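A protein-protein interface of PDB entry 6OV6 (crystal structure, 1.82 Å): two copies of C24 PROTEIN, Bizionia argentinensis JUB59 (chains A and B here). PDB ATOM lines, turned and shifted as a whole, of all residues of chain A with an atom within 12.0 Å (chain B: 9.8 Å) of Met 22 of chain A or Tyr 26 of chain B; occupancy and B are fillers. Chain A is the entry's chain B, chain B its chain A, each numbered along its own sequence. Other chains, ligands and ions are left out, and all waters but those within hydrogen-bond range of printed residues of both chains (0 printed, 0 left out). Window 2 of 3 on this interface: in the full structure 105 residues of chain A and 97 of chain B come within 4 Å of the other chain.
Met 22 of chain A touches Leu 19 of chain B, but with the chains exchanged Leu 19 of chain A does not touch Met 22 of chain B (6.0 Å).
Met 22 of chain B touches its own counterpart, Met 22 of chain A.
Phe 29 of chain A touches Tyr 26 of chain B, but with the chains exchanged Tyr 26 of chain A does not touch Phe 29 of chain B (5.9 Å).
Phe 29 of chain A touches Asn 30 of chain B, but with the chains exchanged Asn 30 of chain A does not touch Phe 29 of chain B (7.9 Å).
Positions printed for both chains: 18, 19, 20, 21, 22, 23, 24, 25, 26, 27, 28, 29, 30, 31 and 32.
OD1 of Asn 30 of chain B sits at hydrogen-bond distance from N of Val 63 of chain B, 3.0 Å away.
O of Ser 27 of chain B is in hydrogen-bond range of ND2 of Asn 30 of chain B (2.9 Å).
Tyr 26 of chain B touches just these residues of chain A: Met 22 (3.3 Å), Ala 25 (3.7 Å), Tyr 26 (3.6 Å) and Phe 29 (3.3 Å).
No residue of chain B comes within 4 Å of Asn 20 of chain A.
Ala 21 of chain A touches none of the printed residues of chain B.
Of chain B, only Tyr 26 (3.7 Å) comes within 4 Å of Ala 25 of chain A.
Leu 19 of chain B touches two residues of chain A.
Gln 23 of chain B touches none of the printed residues of chain A.
No residue of chain A comes within 4 Å of Ala 25 of chain B.
No residue of chain A comes within 4 Å of Val 28 of chain B.
Of the printed residues of chain B, Leu 19 of chain A touches Leu 19.
Of the printed residues of chain B, Tyr 26 of chain A touches Tyr 26.
Of the printed residues of chain A, Leu 32 of chain B touches Leu 32 (3.8 Å).
Of the printed residues of chain B, Leu 32 of chain A touches Phe 29 and Leu 32.
Ser 27 of chain A touches none of the printed residues of chain B.
Lys 65 of chain B touches none of the printed residues of chain A.
The nearest residue of chain B that does not touch Met 22 of chain A is Gln 23 of chain B (5.1 Å).
The nearest printed residue of chain A that does not touch Asn 30 of chain B is Leu 32 of chain A (5.5 Å).
Among the printed residues, merely in contact across the chains: Leu 19 of chain A with Leu 19 of chain B, Met 22 of chain A with Leu 19 of chain B, Met 22 of chain A with Met 22 of chain B, Met 22 of chain A with Tyr 26 of chain B, Ala 25 of chain A with Tyr 26 of chain B, Tyr 26 of chain A with Tyr 26 of chain B, Val 28 of chain A with Val 63 of chain B, Phe 29 of chain A with Tyr 26 of chain B, Phe 29 of chain A with Phe 29 of chain B, Phe 29 of chain A with Asn 30 of chain B, Leu 32 of chain A with Phe 29 of chain B and Leu 32 of chain A with Leu 32 of chain B.
Of the 19 printed residues of chain B, 7 touch a printed residue of chain A.
Printed residues of chain B that touch a printed residue of chain A: Leu 19, Met 22, Tyr 26, Phe 29, Asn 30, Leu 32 and Val 63.
Hydrophobic or aromatic side chains of chain B that line the printed part of chain A: Leu 19, Met 22, Tyr 26, Phe 29, Leu 32 and Val 63.
Of the 15 printed residues of chain A, 7 touch a printed residue of chain B.
Among the printed residues, no Asp or Glu carboxylate lies within 4 Å of a Lys or Arg side-chain nitrogen of the other chain.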
ATOM      1  N   THR A  18      31.119   3.490  34.100  1.00  0.00           N
ATOM      2  CA  THR A  18      30.266   2.325  33.852  1.00  0.00           C
ATOM      3  C   THR A  18      29.646   2.291  32.451  1.00  0.00           C
ATOM      4  O   THR A  18      29.222   1.221  32.012  1.00  0.00           O
ATOM      5  CB  THR A  18      29.237   2.111  34.979  1.00  0.00           C
ATOM      6  OG1 THR A  18      28.593   3.346  35.303  1.00  0.00           O
ATOM      7  CG2 THR A  18      29.851   1.475  36.229  1.00  0.00           C
ATOM      8  N   LEU A  19      29.617   3.444  31.740  1.00  0.00           N
ATOM      9  CA  LEU A  19      29.072   3.563  30.379  1.00  0.00           C
ATOM     10  C   LEU A  19      29.884   2.744  29.360  1.00  0.00           C
ATOM     11  O   LEU A  19      29.332   2.353  28.334  1.00  0.00           O
ATOM     12  CB  LEU A  19      28.941   5.041  29.934  1.00  0.00           C
ATOM     13  CG  LEU A  19      27.886   5.911  30.645  1.00  0.00           C
ATOM     14  CD1 LEU A  19      28.175   7.378  30.444  1.00  0.00           C
ATOM     15  CD2 LEU A  19      26.485   5.618  30.153  1.00  0.00           C
ATOM     16  N   ASN A  20      31.181   2.479  29.657  1.00  0.00           N
ATOM     17  CA  ASN A  20      32.092   1.670  28.839  1.00  0.00           C
ATOM     18  C   ASN A  20      31.623   0.219  28.894  1.00  0.00           C
ATOM     19  O   ASN A  20      31.513  -0.430  27.851  1.00  0.00           O
ATOM     20  CB  ASN A  20      33.518   1.780  29.372  1.00  0.00           C
ATOM     21  N   ALA A  21      31.306  -0.268  30.119  1.00  0.00           N
ATOM     22  CA  ALA A  21      30.774  -1.609  30.383  1.00  0.00           C
ATOM     23  C   ALA A  21      29.347  -1.697  29.819  1.00  0.00           C
ATOM     24  O   ALA A  21      28.941  -2.759  29.349  1.00  0.00           O
ATOM     25  CB  ALA A  21      30.762  -1.879  31.882  1.00  0.00           C
ATOM     26  N   MET A  22      28.626  -0.538  29.824  1.00  0.00           N
ATOM     27  CA  MET A  22      27.263  -0.293  29.324  1.00  0.00           C
ATOM     28  C   MET A  22      27.264   0.236  27.847  1.00  0.00           C
ATOM     29  O   MET A  22      26.514   1.156  27.502  1.00  0.00           O
ATOM     30  CB  MET A  22      26.528   0.684  30.272  1.00  0.00           C
ATOM     31  CG  MET A  22      25.042   0.433  30.411  1.00  0.00           C
ATOM     32  SD  MET A  22      24.159   1.917  30.973  1.00  0.00           S
ATOM     33  CE  MET A  22      23.780   2.671  29.407  1.00  0.00           C
ATOM     34  N   GLN A  23      28.185  -0.303  27.027  1.00  0.00           N
ATOM     35  CA  GLN A  23      28.353  -0.145  25.579  1.00  0.00           C
ATOM     36  C   GLN A  23      28.946  -1.449  25.062  1.00  0.00           C
ATOM     37  O   GLN A  23      28.440  -1.976  24.088  1.00  0.00           O
ATOM     38  CB  GLN A  23      29.226   1.058  25.172  1.00  0.00           C
ATOM     39  CG  GLN A  23      29.289   1.298  23.649  1.00  0.00           C
ATOM     40  CD  GLN A  23      30.623   1.824  23.185  1.00  0.00           C
ATOM     41  OE1 GLN A  23      31.690   1.280  23.505  1.00  0.00           O
ATOM     42  NE2 GLN A  23      30.590   2.885  22.392  1.00  0.00           N
ATOM     43  N   GLU A  24      29.995  -1.987  25.719  1.00  0.00           N
ATOM     44  CA  GLU A  24      30.601  -3.274  25.343  1.00  0.00           C
ATOM     45  C   GLU A  24      29.574  -4.421  25.540  1.00  0.00           C
ATOM     46  O   GLU A  24      29.524  -5.354  24.722  1.00  0.00           O
ATOM     47  CB  GLU A  24      31.854  -3.528  26.172  1.00  0.00           C
ATOM     48  N   ALA A  25      28.722  -4.307  26.600  1.00  0.00           N
ATOM     49  CA  ALA A  25      27.655  -5.270  26.896  1.00  0.00           C
ATOM     50  C   ALA A  25      26.687  -5.382  25.714  1.00  0.00           C
ATOM     51  O   ALA A  25      26.450  -6.495  25.238  1.00  0.00           O
ATOM     52  CB  ALA A  25      26.901  -4.879  28.162  1.00  0.00           C
ATOM     53  N   TYR A  26      26.170  -4.243  25.217  1.00  0.00           N
ATOM     54  CA  TYR A  26      25.265  -4.281  24.074  1.00  0.00           C
ATOM     55  C   TYR A  26      25.934  -4.497  22.709  1.00  0.00           C
ATOM     56  O   TYR A  26      25.262  -4.971  21.785  1.00  0.00           O
ATOM     57  CB  TYR A  26      24.162  -3.184  24.089  1.00  0.00           C
ATOM     58  CG  TYR A  26      24.595  -1.780  23.747  1.00  0.00           C
ATOM     59  CD1 TYR A  26      24.925  -1.432  22.444  1.00  0.00           C
ATOM     60  CD2 TYR A  26      24.578  -0.774  24.706  1.00  0.00           C
ATOM     61  CE1 TYR A  26      25.306  -0.137  22.119  1.00  0.00           C
ATOM     62  CE2 TYR A  26      24.953   0.528  24.391  1.00  0.00           C
ATOM     63  CZ  TYR A  26      25.303   0.843  23.093  1.00  0.00           C
ATOM     64  OH  TYR A  26      25.685   2.118  22.768  1.00  0.00           O
ATOM     65  N   SER A  27      27.250  -4.201  22.573  1.00  0.00           N
ATOM     66  CA  SER A  27      27.957  -4.393  21.301  1.00  0.00           C
ATOM     67  C   SER A  27      27.951  -5.865  20.812  1.00  0.00           C
ATOM     68  O   SER A  27      27.984  -6.080  19.596  1.00  0.00           O
ATOM     69  CB  SER A  27      29.402  -3.904  21.411  1.00  0.00           C
ATOM     70  OG  SER A  27      29.494  -2.506  21.657  1.00  0.00           O
ATOM     71  N   VAL A  28      27.878  -6.873  21.754  1.00  0.00           N
ATOM     72  CA  VAL A  28      27.870  -8.338  21.472  1.00  0.00           C
ATOM     73  C   VAL A  28      26.639  -8.749  20.626  1.00  0.00           C
ATOM     74  O   VAL A  28      26.630  -9.808  19.971  1.00  0.00           O
ATOM     75  CB  VAL A  28      28.009  -9.201  22.772  1.00  0.00           C
ATOM     76  CG1 VAL A  28      26.678  -9.361  23.507  1.00  0.00           C
ATOM     77  CG2 VAL A  28      28.638 -10.556  22.478  1.00  0.00           C
ATOM     78  N   PHE A  29      25.615  -7.903  20.647  1.00  0.00           N
ATOM     79  CA  PHE A  29      24.398  -8.138  19.882  1.00  0.00           C
ATOM     80  C   PHE A  29      24.591  -8.046  18.372  1.00  0.00           C
ATOM     81  O   PHE A  29      23.844  -8.678  17.635  1.00  0.00           O
ATOM     82  CB  PHE A  29      23.195  -7.350  20.425  1.00  0.00           C
ATOM     83  CG  PHE A  29      22.877  -7.646  21.881  1.00  0.00           C
ATOM     84  CD1 PHE A  29      22.748  -8.953  22.336  1.00  0.00           C
ATOM     85  CD2 PHE A  29      22.674  -6.617  22.784  1.00  0.00           C
ATOM     86  CE1 PHE A  29      22.458  -9.223  23.672  1.00  0.00           C
ATOM     87  CE2 PHE A  29      22.371  -6.891  24.123  1.00  0.00           C
ATOM     88  CZ  PHE A  29      22.253  -8.196  24.552  1.00  0.00           C
ATOM     89  N   ASN A  30      25.671  -7.352  17.902  1.00  0.00           N
ATOM     90  CA  ASN A  30      26.012  -7.326  16.490  1.00  0.00           C
ATOM     91  C   ASN A  30      26.218  -8.753  15.966  1.00  0.00           C
ATOM     92  O   ASN A  30      25.867  -9.036  14.826  1.00  0.00           O
ATOM     93  CB  ASN A  30      27.288  -6.513  16.258  1.00  0.00           C
ATOM     94  CG  ASN A  30      26.982  -5.062  16.022  1.00  0.00           C
ATOM     95  OD1 ASN A  30      26.403  -4.687  14.994  1.00  0.00           O
ATOM     96  ND2 ASN A  30      27.276  -4.236  17.012  1.00  0.00           N
ATOM     97  N   ALA A  31      26.828  -9.640  16.793  1.00  0.00           N
ATOM     98  CA  ALA A  31      27.106 -11.022  16.397  1.00  0.00           C
ATOM     99  C   ALA A  31      25.837 -11.834  16.097  1.00  0.00           C
ATOM    100  O   ALA A  31      25.908 -12.807  15.346  1.00  0.00           O
ATOM    101  CB  ALA A  31      27.943 -11.713  17.467  1.00  0.00           C
ATOM    102  N   LEU A  32      24.674 -11.412  16.641  1.00  0.00           N
ATOM    103  CA  LEU A  32      23.388 -12.090  16.373  1.00  0.00           C
ATOM    104  C   LEU A  32      22.995 -11.991  14.893  1.00  0.00           C
ATOM    105  O   LEU A  32      22.204 -12.788  14.407  1.00  0.00           O
ATOM    106  CB  LEU A  32      22.268 -11.551  17.271  1.00  0.00           C
ATOM    107  CG  LEU A  32      22.378 -11.870  18.771  1.00  0.00           C
ATOM    108  CD1 LEU A  32      21.386 -11.026  19.546  1.00  0.00           C
ATOM    109  CD2 LEU A  32      22.103 -13.358  19.086  1.00  0.00           C
ATOM    110  N   THR B  18      17.470   6.483  34.908  1.00  0.00           N
ATOM    111  CA  THR B  18      17.294   6.254  33.474  1.00  0.00           C
ATOM    112  C   THR B  18      18.298   5.248  32.883  1.00  0.00           C
ATOM    113  O   THR B  18      17.976   4.593  31.883  1.00  0.00           O
ATOM    114  CB  THR B  18      17.134   7.568  32.677  1.00  0.00           C
ATOM    115  OG1 THR B  18      18.210   8.464  32.971  1.00  0.00           O
ATOM    116  CG2 THR B  18      15.786   8.247  32.930  1.00  0.00           C
ATOM    117  N   LEU B  19      19.494   5.093  33.513  1.00  0.00           N
ATOM    118  CA  LEU B  19      20.467   4.082  33.060  1.00  0.00           C
ATOM    119  C   LEU B  19      19.953   2.649  33.371  1.00  0.00           C
ATOM    120  O   LEU B  19      20.358   1.701  32.687  1.00  0.00           O
ATOM    121  CB  LEU B  19      21.883   4.309  33.622  1.00  0.00           C
ATOM    122  CG  LEU B  19      22.617   5.592  33.184  1.00  0.00           C
ATOM    123  CD1 LEU B  19      23.807   5.877  34.101  1.00  0.00           C
ATOM    124  CD2 LEU B  19      23.077   5.527  31.713  1.00  0.00           C
ATOM    125  N   ASN B  20      19.044   2.518  34.394  1.00  0.00           N
ATOM    126  CA  ASN B  20      18.340   1.290  34.791  1.00  0.00           C
ATOM    127  C   ASN B  20      17.410   0.885  33.630  1.00  0.00           C
ATOM    128  O   ASN B  20      17.433  -0.269  33.180  1.00  0.00           O
ATOM    129  CB  ASN B  20      17.483   1.506  36.062  1.00  0.00           C
ATOM    130  CG  ASN B  20      18.216   1.672  37.386  1.00  0.00           C
ATOM    131  OD1 ASN B  20      19.332   2.206  37.463  1.00  0.00           O
ATOM    132  ND2 ASN B  20      17.538   1.334  38.482  1.00  0.00           N
ATOM    133  N   ALA B  21      16.617   1.868  33.132  1.00  0.00           N
ATOM    134  CA  ALA B  21      15.697   1.703  32.002  1.00  0.00           C
ATOM    135  C   ALA B  21      16.483   1.413  30.722  1.00  0.00           C
ATOM    136  O   ALA B  21      16.015   0.636  29.899  1.00  0.00           O
ATOM    137  CB  ALA B  21      14.837   2.954  31.835  1.00  0.00           C
ATOM    138  N   MET B  22      17.685   1.984  30.586  1.00  0.00           N
ATOM    139  CA  MET B  22      18.576   1.773  29.457  1.00  0.00           C
ATOM    140  C   MET B  22      19.100   0.327  29.387  1.00  0.00           C
ATOM    141  O   MET B  22      19.118  -0.274  28.300  1.00  0.00           O
ATOM    142  CB  MET B  22      19.753   2.735  29.534  1.00  0.00           C
ATOM    143  CG  MET B  22      20.258   3.141  28.179  1.00  0.00           C
ATOM    144  SD  MET B  22      20.877   4.853  28.152  1.00  0.00           S
ATOM    145  CE  MET B  22      19.555   5.705  29.011  1.00  0.00           C
ATOM    146  N   GLN B  23      19.574  -0.200  30.549  1.00  0.00           N
ATOM    147  CA  GLN B  23      20.144  -1.534  30.673  1.00  0.00           C
ATOM    148  C   GLN B  23      19.044  -2.546  30.447  1.00  0.00           C
ATOM    149  O   GLN B  23      19.247  -3.504  29.702  1.00  0.00           O
ATOM    150  CB  GLN B  23      20.776  -1.750  32.068  1.00  0.00           C
ATOM    151  CG  GLN B  23      21.511  -3.116  32.213  1.00  0.00           C
ATOM    152  CD  GLN B  23      21.334  -3.826  33.552  1.00  0.00           C
ATOM    153  OE1 GLN B  23      20.342  -3.634  34.283  1.00  0.00           O
ATOM    154  NE2 GLN B  23      22.303  -4.689  33.906  1.00  0.00           N
ATOM    155  N   GLU B  24      17.887  -2.317  31.088  1.00  0.00           N
ATOM    156  CA  GLU B  24      16.702  -3.172  30.987  1.00  0.00           C
ATOM    157  C   GLU B  24      16.243  -3.230  29.550  1.00  0.00           C
ATOM    158  O   GLU B  24      15.813  -4.302  29.087  1.00  0.00           O
ATOM    159  CB  GLU B  24      15.567  -2.673  31.899  1.00  0.00           C
ATOM    160  CG  GLU B  24      15.676  -3.136  33.349  1.00  0.00           C
ATOM    161  CD  GLU B  24      14.629  -2.548  34.279  1.00  0.00           C
ATOM    162  OE1 GLU B  24      13.417  -2.684  33.985  1.00  0.00           O
ATOM    163  OE2 GLU B  24      15.019  -1.955  35.310  1.00  0.00           O
ATOM    164  N   ALA B  25      16.400  -2.091  28.827  1.00  0.00           N
ATOM    165  CA  ALA B  25      16.042  -1.966  27.417  1.00  0.00           C
ATOM    166  C   ALA B  25      16.927  -2.849  26.575  1.00  0.00           C
ATOM    167  O   ALA B  25      16.398  -3.763  25.965  1.00  0.00           O
ATOM    168  CB  ALA B  25      16.124  -0.518  26.948  1.00  0.00           C
ATOM    169  N   TYR B  26      18.264  -2.644  26.586  1.00  0.00           N
ATOM    170  CA  TYR B  26      19.134  -3.488  25.759  1.00  0.00           C
ATOM    171  C   TYR B  26      19.235  -4.952  26.214  1.00  0.00           C
ATOM    172  O   TYR B  26      19.532  -5.808  25.376  1.00  0.00           O
ATOM    173  CB  TYR B  26      20.512  -2.854  25.425  1.00  0.00           C
ATOM    174  CG  TYR B  26      21.514  -2.802  26.568  1.00  0.00           C
ATOM    175  CD1 TYR B  26      22.165  -3.951  27.003  1.00  0.00           C
ATOM    176  CD2 TYR B  26      21.884  -1.586  27.148  1.00  0.00           C
ATOM    177  CE1 TYR B  26      23.081  -3.916  28.052  1.00  0.00           C
ATOM    178  CE2 TYR B  26      22.811  -1.535  28.196  1.00  0.00           C
ATOM    179  CZ  TYR B  26      23.413  -2.707  28.638  1.00  0.00           C
ATOM    180  OH  TYR B  26      24.320  -2.698  29.674  1.00  0.00           O
ATOM    181  N   SER B  27      19.001  -5.238  27.537  1.00  0.00           N
ATOM    182  CA  SER B  27      19.120  -6.621  28.023  1.00  0.00           C
ATOM    183  C   SER B  27      18.133  -7.557  27.337  1.00  0.00           C
ATOM    184  O   SER B  27      18.431  -8.753  27.190  1.00  0.00           O
ATOM    185  CB  SER B  27      18.999  -6.709  29.540  1.00  0.00           C
ATOM    186  OG  SER B  27      17.735  -6.230  29.956  1.00  0.00           O
ATOM    187  N   VAL B  28      16.977  -7.017  26.872  1.00  0.00           N
ATOM    188  CA  VAL B  28      15.969  -7.841  26.167  1.00  0.00           C
ATOM    189  C   VAL B  28      16.544  -8.522  24.919  1.00  0.00           C
ATOM    190  O   VAL B  28      16.040  -9.593  24.564  1.00  0.00           O
ATOM    191  CB  VAL B  28      14.626  -7.089  25.865  1.00  0.00           C
ATOM    192  CG1 VAL B  28      14.749  -6.180  24.631  1.00  0.00           C
ATOM    193  CG2 VAL B  28      13.475  -8.085  25.670  1.00  0.00           C
ATOM    194  N   PHE B  29      17.609  -7.939  24.278  1.00  0.00           N
ATOM    195  CA  PHE B  29      18.215  -8.497  23.064  1.00  0.00           C
ATOM    196  C   PHE B  29      18.874  -9.842  23.267  1.00  0.00           C
ATOM    197  O   PHE B  29      18.989 -10.601  22.305  1.00  0.00           O
ATOM    198  CB  PHE B  29      19.102  -7.479  22.319  1.00  0.00           C
ATOM    199  CG  PHE B  29      18.361  -6.209  21.953  1.00  0.00           C
ATOM    200  CD1 PHE B  29      17.173  -6.261  21.223  1.00  0.00           C
ATOM    201  CD2 PHE B  29      18.876  -4.955  22.299  1.00  0.00           C
ATOM    202  CE1 PHE B  29      16.486  -5.085  20.877  1.00  0.00           C
ATOM    203  CE2 PHE B  29      18.202  -3.782  21.936  1.00  0.00           C
ATOM    204  CZ  PHE B  29      17.023  -3.852  21.216  1.00  0.00           C
ATOM    205  N   ASN B  30      19.208 -10.189  24.519  1.00  0.00           N
ATOM    206  CA  ASN B  30      19.759 -11.521  24.813  1.00  0.00           C
ATOM    207  C   ASN B  30      18.757 -12.574  24.440  1.00  0.00           C
ATOM    208  O   ASN B  30      19.165 -13.640  23.992  1.00  0.00           O
ATOM    209  CB  ASN B  30      20.068 -11.668  26.299  1.00  0.00           C
ATOM    210  CG  ASN B  30      21.314 -10.955  26.692  1.00  0.00           C
ATOM    211  OD1 ASN B  30      22.419 -11.384  26.346  1.00  0.00           O
ATOM    212  ND2 ASN B  30      21.153  -9.840  27.410  1.00  0.00           N
ATOM    213  N   ALA B  31      17.437 -12.291  24.628  1.00  0.00           N
ATOM    214  CA  ALA B  31      16.368 -13.242  24.288  1.00  0.00           C
ATOM    215  C   ALA B  31      16.432 -13.683  22.821  1.00  0.00           C
ATOM    216  O   ALA B  31      16.004 -14.785  22.515  1.00  0.00           O
ATOM    217  CB  ALA B  31      14.988 -12.675  24.629  1.00  0.00           C
ATOM    218  N   LEU B  32      17.013 -12.860  21.931  1.00  0.00           N
ATOM    219  CA  LEU B  32      17.202 -13.194  20.508  1.00  0.00           C
ATOM    220  C   LEU B  32      18.054 -14.442  20.299  1.00  0.00           C
ATOM    221  O   LEU B  32      17.933 -15.099  19.259  1.00  0.00           O
ATOM    222  CB  LEU B  32      17.692 -11.995  19.664  1.00  0.00           C
ATOM    223  CG  LEU B  32      16.710 -10.794  19.559  1.00  0.00           C
ATOM    224  CD1 LEU B  32      17.416  -9.558  19.099  1.00  0.00           C
ATOM    225  CD2 LEU B  32      15.532 -11.089  18.636  1.00  0.00           C
ATOM    226  N   GLY B  61      19.967 -17.949  28.388  1.00  0.00           N
ATOM    227  CA  GLY B  61      19.468 -16.593  28.259  1.00  0.00           C
ATOM    228  C   GLY B  61      20.497 -15.502  28.078  1.00  0.00           C
ATOM    229  O   GLY B  61      20.115 -14.340  28.025  1.00  0.00           O
ATOM    230  N   VAL B  63      23.969 -13.955  25.849  1.00  0.00           N
ATOM    231  CA  VAL B  63      24.861 -13.963  24.700  1.00  0.00           C
ATOM    232  C   VAL B  63      26.254 -13.628  25.264  1.00  0.00           C
ATOM    233  O   VAL B  63      26.405 -12.597  25.942  1.00  0.00           O
ATOM    234  CB  VAL B  63      24.421 -12.949  23.606  1.00  0.00           C
ATOM    235  CG1 VAL B  63      25.425 -12.889  22.458  1.00  0.00           C
ATOM    236  CG2 VAL B  63      23.016 -13.237  23.085  1.00  0.00           C
ATOM    237  N   LYS B  65      30.725 -13.487  24.626  1.00  0.00           N
ATOM    238  CA  LYS B  65      31.947 -13.577  23.838  1.00  0.00           C
ATOM    239  C   LYS B  65      32.572 -14.925  24.281  1.00  0.00           C
ATOM    240  O   LYS B  65      32.501 -15.284  25.467  1.00  0.00           O
ATOM    241  CB  LYS B  65      32.932 -12.442  24.185  1.00  0.00           C
ATOM    242  CG  LYS B  65      32.538 -11.084  23.612  1.00  0.00           C
ATOM    243  CD  LYS B  65      33.240  -9.924  24.323  1.00  0.00           C
ATOM    244  CE  LYS B  65      32.602  -8.589  23.997  1.00  0.00           C
ATOM    245  NZ  LYS B  65      33.207  -7.485  24.786  1.00  0.00           N
ATOM    246  N   PHE B  96      34.979  -6.617  36.862  1.00  0.00           N
ATOM    247  CA  PHE B  96      34.968  -7.917  36.190  1.00  0.00           C
ATOM    248  C   PHE B  96      34.209  -7.924  34.874  1.00  0.00           C
ATOM    249  O   PHE B  96      33.270  -7.149  34.684  1.00  0.00           O
ATOM    250  CB  PHE B  96      34.382  -8.988  37.124  1.00  0.00           C
ATOM    251  CG  PHE B  96      35.136  -9.225  38.408  1.00  0.00           C
ATOM    252  CD1 PHE B  96      36.325  -9.949  38.412  1.00  0.00           C
ATOM    253  CD2 PHE B  96      34.659  -8.722  39.616  1.00  0.00           C
ATOM    254  CE1 PHE B  96      37.045 -10.140  39.597  1.00  0.00           C
ATOM    255  CE2 PHE B  96      35.360  -8.944  40.807  1.00  0.00           C
ATOM    256  CZ  PHE B  96      36.547  -9.657  40.789  1.00  0.00           C
